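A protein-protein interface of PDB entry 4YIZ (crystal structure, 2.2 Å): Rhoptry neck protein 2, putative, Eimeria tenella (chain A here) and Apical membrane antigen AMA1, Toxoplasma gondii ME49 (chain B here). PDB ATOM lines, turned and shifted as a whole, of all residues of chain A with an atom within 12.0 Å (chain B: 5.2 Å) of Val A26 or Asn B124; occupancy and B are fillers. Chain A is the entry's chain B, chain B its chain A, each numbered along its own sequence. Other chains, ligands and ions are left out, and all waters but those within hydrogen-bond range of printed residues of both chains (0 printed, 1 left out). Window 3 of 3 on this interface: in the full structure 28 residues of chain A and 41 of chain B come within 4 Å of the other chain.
Of chain B, only Asn B124 (3.8 Å), Ile B127 (3.7 Å) and Phe B139 (3.97 Å) come within 4 Å of Val A26.
No residue of chain A comes within 4 Å of Leu B121.
No residue of chain A comes within 4 Å of Lys B123.
No residue of chain A comes within 4 Å of Ser B125.
Of the printed residues of chain A, Phe B139 touches Asn A24 and Val A26.
Of the printed residues of chain B, Asn A24 touches Phe B139 (3.4 Å).
Printed residues of chain B within 4 Å of Leu A25: Asn B126 (3.6 Å).
Printed residues of chain A within 4 Å of Phe B116: Val A27 (3.9 Å).
Leu A22 touches none of the printed residues of chain B.
Gly A28 touches none of the printed residues of chain B.
The nearest residue of chain B that does not touch Val A26 is Asn B126 (4.04 Å).
The nearest residue of chain A that does not touch Asn B124 is Leu A25 (6.3 Å).
The nearest printed residue of chain B that does not touch Leu A25 is Asn B124 (6.3 Å).
Printed residues of chain A that touch a printed residue of chain B: Asn A24, Leu A25, Val A26 and Val A27.
Hydrophobic or aromatic side chains of chain A that line the printed part of chain B: Val A26 and Val A27.
Along chain A the printed residues that touch a printed residue of chain B span positions 24 to 27.
Of the 10 printed residues of chain B, 5 touch a printed residue of chain A.
Hydrophobic or aromatic side chains of chain B within 4 Å of the printed part of chain A: Phe B116, Ile B127 and Phe B139.
Among the printed residues, no Asp or Glu carboxylate lies within 4 Å of a Lys or Arg side-chain nitrogen of the other chain.
Asn A24 touches Phe B139.
Asn B126 touches Leu A25 (OD1 to O, 3.6 Å).
ND2 of Asn B124 touches CG1 of Val A26 (3.8 Å).
Ile B127 touches Val A26 (CD1 to CG2, 3.7 Å).
CG2 of Val A26 touches CD1 of Phe B139, at 3.97 Å.
Val A27 touches Phe B116 (CG1 to CE1, 3.9 Å).
The side-chain amide nitrogen (ND2) of Asn B126 is in hydrogen-bond range of the side-chain amide oxygen (OD1) of Asn B124, 2.9 Å away.
The side-chain hydroxyl (OG) of Ser B125 sits at hydrogen-bond distance from the side-chain amide nitrogen (ND2) of Asn B126 (3.3 Å).
N of Val A27 lies within hydrogen-bond range of OD1 of Asn A24.
N of Val A26 lies within hydrogen-bond range of OD1 of Asn A24.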
ATOM      1  N   LEU A  22      10.250  -9.170 -16.547  1.00  0.00           N
ATOM      2  CA  LEU A  22      10.587  -9.368 -15.139  1.00  0.00           C
ATOM      3  C   LEU A  22      10.508 -10.860 -14.843  1.00  0.00           C
ATOM      4  O   LEU A  22       9.660 -11.555 -15.396  1.00  0.00           O
ATOM      5  CB  LEU A  22       9.646  -8.583 -14.219  1.00  0.00           C
ATOM      6  CG  LEU A  22      10.093  -7.198 -13.740  1.00  0.00           C
ATOM      7  CD1 LEU A  22      10.583  -6.328 -14.881  1.00  0.00           C
ATOM      8  CD2 LEU A  22       8.946  -6.515 -13.017  1.00  0.00           C
ATOM      9  N   GLU A  23      11.396 -11.350 -13.983  1.00  0.00           N
ATOM     10  CA  GLU A  23      11.360 -12.744 -13.550  1.00  0.00           C
ATOM     11  C   GLU A  23      10.850 -12.837 -12.117  1.00  0.00           C
ATOM     12  O   GLU A  23      11.429 -12.239 -11.209  1.00  0.00           O
ATOM     13  CB  GLU A  23      12.747 -13.387 -13.657  1.00  0.00           C
ATOM     14  CG  GLU A  23      12.811 -14.837 -13.177  1.00  0.00           C
ATOM     15  CD  GLU A  23      11.901 -15.762 -13.965  1.00  0.00           C
ATOM     16  OE1 GLU A  23      11.558 -15.424 -15.118  1.00  0.00           O
ATOM     17  OE2 GLU A  23      11.527 -16.829 -13.431  1.00  0.00           O
ATOM     18  N   ASN A  24       9.762 -13.577 -11.926  1.00  0.00           N
ATOM     19  CA  ASN A  24       9.216 -13.810 -10.595  1.00  0.00           C
ATOM     20  C   ASN A  24       9.211 -15.298 -10.267  1.00  0.00           C
ATOM     21  O   ASN A  24       8.820 -16.122 -11.092  1.00  0.00           O
ATOM     22  CB  ASN A  24       7.806 -13.237 -10.491  1.00  0.00           C
ATOM     23  CG  ASN A  24       7.154 -13.543  -9.164  1.00  0.00           C
ATOM     24  OD1 ASN A  24       6.564 -14.605  -8.981  1.00  0.00           O
ATOM     25  ND2 ASN A  24       7.258 -12.610  -8.225  1.00  0.00           N
ATOM     26  N   LEU A  25       9.685 -15.640  -9.085  1.00  0.00           N
ATOM     27  CA  LEU A  25       9.794 -17.025  -8.653  1.00  0.00           C
ATOM     28  C   LEU A  25       8.484 -17.764  -8.483  1.00  0.00           C
ATOM     29  O   LEU A  25       8.445 -18.975  -8.528  1.00  0.00           O
ATOM     30  CB  LEU A  25      10.651 -17.144  -7.396  1.00  0.00           C
ATOM     31  CG  LEU A  25      12.012 -16.460  -7.477  1.00  0.00           C
ATOM     32  CD1 LEU A  25      12.862 -16.705  -6.247  1.00  0.00           C
ATOM     33  CD2 LEU A  25      12.755 -16.844  -8.739  1.00  0.00           C
ATOM     34  N   VAL A  26       7.416 -17.034  -8.258  1.00  0.00           N
ATOM     35  CA  VAL A  26       6.113 -17.655  -8.035  1.00  0.00           C
ATOM     36  C   VAL A  26       5.374 -17.909  -9.353  1.00  0.00           C
ATOM     37  O   VAL A  26       4.773 -18.970  -9.531  1.00  0.00           O
ATOM     38  CB  VAL A  26       5.226 -16.787  -7.115  1.00  0.00           C
ATOM     39  CG1 VAL A  26       3.844 -17.403  -6.958  1.00  0.00           C
ATOM     40  CG2 VAL A  26       5.882 -16.627  -5.754  1.00  0.00           C
ATOM     41  N   VAL A  27       5.429 -16.943 -10.269  1.00  0.00           N
ATOM     42  CA  VAL A  27       4.651 -17.000 -11.508  1.00  0.00           C
ATOM     43  C   VAL A  27       5.522 -17.064 -12.763  1.00  0.00           C
ATOM     44  O   VAL A  27       5.005 -17.103 -13.880  1.00  0.00           O
ATOM     45  CB  VAL A  27       3.704 -15.782 -11.628  1.00  0.00           C
ATOM     46  CG1 VAL A  27       2.790 -15.707 -10.414  1.00  0.00           C
ATOM     47  CG2 VAL A  27       4.488 -14.478 -11.787  1.00  0.00           C
ATOM     48  N   GLY A  28       6.839 -17.071 -12.582  1.00  0.00           N
ATOM     49  CA  GLY A  28       7.758 -17.139 -13.704  1.00  0.00           C
ATOM     50  C   GLY A  28       8.001 -15.782 -14.341  1.00  0.00           C
ATOM     51  O   GLY A  28       7.844 -14.750 -13.687  1.00  0.00           O
ATOM     52  N   PRO A  29       8.413 -15.776 -15.619  1.00  0.00           N
ATOM     53  CA  PRO A  29       8.624 -14.517 -16.338  1.00  0.00           C
ATOM     54  C   PRO A  29       7.323 -13.806 -16.691  1.00  0.00           C
ATOM     55  O   PRO A  29       6.328 -14.454 -17.017  1.00  0.00           O
ATOM     56  CB  PRO A  29       9.366 -14.952 -17.607  1.00  0.00           C
ATOM     57  CG  PRO A  29       9.032 -16.384 -17.774  1.00  0.00           C
ATOM     58  CD  PRO A  29       8.888 -16.934 -16.395  1.00  0.00           C
ATOM     59  N   VAL A  30       7.345 -12.478 -16.621  1.00  0.00           N
ATOM     60  CA  VAL A  30       6.194 -11.666 -16.977  1.00  0.00           C
ATOM     61  C   VAL A  30       6.630 -10.502 -17.856  1.00  0.00           C
ATOM     62  O   VAL A  30       7.709  -9.925 -17.668  1.00  0.00           O
ATOM     63  CB  VAL A  30       5.456 -11.135 -15.732  1.00  0.00           C
ATOM     64  CG1 VAL A  30       4.817 -12.286 -14.971  1.00  0.00           C
ATOM     65  CG2 VAL A  30       6.400 -10.347 -14.829  1.00  0.00           C
ATOM     66  N   PHE B 116      -1.577  -8.700  -6.686  1.00  0.00           N
ATOM     67  CA  PHE B 116      -1.559 -10.140  -6.464  1.00  0.00           C
ATOM     68  C   PHE B 116      -2.269 -10.480  -5.154  1.00  0.00           C
ATOM     69  O   PHE B 116      -1.933  -9.924  -4.112  1.00  0.00           O
ATOM     70  CB  PHE B 116      -0.122 -10.650  -6.437  1.00  0.00           C
ATOM     71  CG  PHE B 116       0.005 -12.111  -6.737  1.00  0.00           C
ATOM     72  CD1 PHE B 116      -0.036 -12.564  -8.044  1.00  0.00           C
ATOM     73  CD2 PHE B 116       0.168 -13.032  -5.716  1.00  0.00           C
ATOM     74  CE1 PHE B 116       0.080 -13.908  -8.328  1.00  0.00           C
ATOM     75  CE2 PHE B 116       0.285 -14.379  -5.994  1.00  0.00           C
ATOM     76  CZ  PHE B 116       0.241 -14.818  -7.301  1.00  0.00           C
ATOM     77  N   LEU B 120      -3.350 -16.474  -2.584  1.00  0.00           N
ATOM     78  CA  LEU B 120      -2.499 -17.287  -3.448  1.00  0.00           C
ATOM     79  C   LEU B 120      -1.061 -17.361  -2.939  1.00  0.00           C
ATOM     80  O   LEU B 120      -0.267 -18.163  -3.431  1.00  0.00           O
ATOM     81  CB  LEU B 120      -2.519 -16.736  -4.874  1.00  0.00           C
ATOM     82  CG  LEU B 120      -3.623 -17.284  -5.785  1.00  0.00           C
ATOM     83  CD1 LEU B 120      -4.987 -17.257  -5.101  1.00  0.00           C
ATOM     84  CD2 LEU B 120      -3.663 -16.494  -7.088  1.00  0.00           C
ATOM     85  N   LEU B 121      -0.734 -16.532  -1.951  1.00  0.00           N
ATOM     86  CA  LEU B 121       0.616 -16.493  -1.397  1.00  0.00           C
ATOM     87  C   LEU B 121       0.713 -17.278  -0.094  1.00  0.00           C
ATOM     88  O   LEU B 121       1.752 -17.860   0.208  1.00  0.00           O
ATOM     89  CB  LEU B 121       1.056 -15.046  -1.157  1.00  0.00           C
ATOM     90  CG  LEU B 121       1.286 -14.176  -2.396  1.00  0.00           C
ATOM     91  CD1 LEU B 121       1.576 -12.739  -1.982  1.00  0.00           C
ATOM     92  CD2 LEU B 121       2.420 -14.721  -3.250  1.00  0.00           C
ATOM     93  N   GLU B 122      -0.374 -17.302   0.667  1.00  0.00           N
ATOM     94  CA  GLU B 122      -0.325 -17.817   2.032  1.00  0.00           C
ATOM     95  C   GLU B 122      -0.347 -19.347   2.116  1.00  0.00           C
ATOM     96  O   GLU B 122      -0.285 -19.903   3.212  1.00  0.00           O
ATOM     97  CB  GLU B 122      -1.478 -17.227   2.854  1.00  0.00           C
ATOM     98  CG  GLU B 122      -2.869 -17.486   2.300  1.00  0.00           C
ATOM     99  CD  GLU B 122      -3.946 -16.727   3.057  1.00  0.00           C
ATOM    100  OE1 GLU B 122      -3.596 -15.940   3.963  1.00  0.00           O
ATOM    101  OE2 GLU B 122      -5.142 -16.917   2.749  1.00  0.00           O
ATOM    102  N   LYS B 123      -0.419 -20.021   0.970  1.00  0.00           N
ATOM    103  CA  LYS B 123      -0.319 -21.481   0.928  1.00  0.00           C
ATOM    104  C   LYS B 123       0.558 -21.931  -0.241  1.00  0.00           C
ATOM    105  O   LYS B 123       0.371 -23.019  -0.787  1.00  0.00           O
ATOM    106  CB  LYS B 123      -1.707 -22.121   0.816  1.00  0.00           C
ATOM    107  CG  LYS B 123      -2.630 -21.840   1.999  1.00  0.00           C
ATOM    108  CD  LYS B 123      -4.095 -22.036   1.634  1.00  0.00           C
ATOM    109  CE  LYS B 123      -4.598 -20.942   0.699  1.00  0.00           C
ATOM    110  NZ  LYS B 123      -5.352 -19.877   1.414  1.00  0.00           N
ATOM    111  N   ASN B 124       1.518 -21.090  -0.611  1.00  0.00           N
ATOM    112  CA  ASN B 124       2.404 -21.368  -1.738  1.00  0.00           C
ATOM    113  C   ASN B 124       3.765 -21.883  -1.264  1.00  0.00           C
ATOM    114  O   ASN B 124       4.151 -21.664  -0.114  1.00  0.00           O
ATOM    115  CB  ASN B 124       2.579 -20.108  -2.588  1.00  0.00           C
ATOM    116  CG  ASN B 124       3.231 -20.392  -3.929  1.00  0.00           C
ATOM    117  OD1 ASN B 124       4.433 -20.631  -4.006  1.00  0.00           O
ATOM    118  ND2 ASN B 124       2.438 -20.358  -4.993  1.00  0.00           N
ATOM    119  N   SER B 125       4.487 -22.566  -2.153  1.00  0.00           N
ATOM    120  CA  SER B 125       5.768 -23.194  -1.803  1.00  0.00           C
ATOM    121  C   SER B 125       6.902 -22.183  -1.735  1.00  0.00           C
ATOM    122  O   SER B 125       7.719 -22.207  -0.815  1.00  0.00           O
ATOM    123  CB  SER B 125       6.132 -24.287  -2.818  1.00  0.00           C
ATOM    124  OG  SER B 125       6.909 -23.775  -3.887  1.00  0.00           O
ATOM    125  N   ASN B 126       6.940 -21.296  -2.723  1.00  0.00           N
ATOM    126  CA  ASN B 126       8.013 -20.320  -2.851  1.00  0.00           C
ATOM    127  C   ASN B 126       7.923 -19.186  -1.827  1.00  0.00           C
ATOM    128  O   ASN B 126       8.734 -18.263  -1.853  1.00  0.00           O
ATOM    129  CB  ASN B 126       8.005 -19.726  -4.265  1.00  0.00           C
ATOM    130  CG  ASN B 126       7.897 -20.787  -5.351  1.00  0.00           C
ATOM    131  OD1 ASN B 126       8.904 -21.331  -5.805  1.00  0.00           O
ATOM    132  ND2 ASN B 126       6.673 -21.074  -5.782  1.00  0.00           N
ATOM    133  N   ILE B 127       6.941 -19.260  -0.931  1.00  0.00           N
ATOM    134  CA  ILE B 127       6.682 -18.191   0.030  1.00  0.00           C
ATOM    135  C   ILE B 127       6.714 -18.730   1.459  1.00  0.00           C
ATOM    136  O   ILE B 127       5.838 -19.496   1.858  1.00  0.00           O
ATOM    137  CB  ILE B 127       5.319 -17.524  -0.236  1.00  0.00           C
ATOM    138  CG1 ILE B 127       5.212 -17.071  -1.698  1.00  0.00           C
ATOM    139  CG2 ILE B 127       5.106 -16.354   0.709  1.00  0.00           C
ATOM    140  CD1 ILE B 127       6.187 -15.978  -2.091  1.00  0.00           C
ATOM    141  N   PHE B 139       7.267 -11.695  -1.864  1.00  0.00           N
ATOM    142  CA  PHE B 139       6.839 -11.712  -3.256  1.00  0.00           C
ATOM    143  C   PHE B 139       7.585 -10.645  -4.043  1.00  0.00           C
ATOM    144  O   PHE B 139       8.086 -10.906  -5.139  1.00  0.00           O
ATOM    145  CB  PHE B 139       5.329 -11.495  -3.355  1.00  0.00           C
ATOM    146  CG  PHE B 139       4.784 -11.613  -4.750  1.00  0.00           C
ATOM    147  CD1 PHE B 139       4.757 -12.836  -5.397  1.00  0.00           C
ATOM    148  CD2 PHE B 139       4.277 -10.502  -5.405  1.00  0.00           C
ATOM    149  CE1 PHE B 139       4.249 -12.947  -6.676  1.00  0.00           C
ATOM    150  CE2 PHE B 139       3.767 -10.607  -6.685  1.00  0.00           C
ATOM    151  CZ  PHE B 139       3.753 -11.832  -7.322  1.00  0.00           C
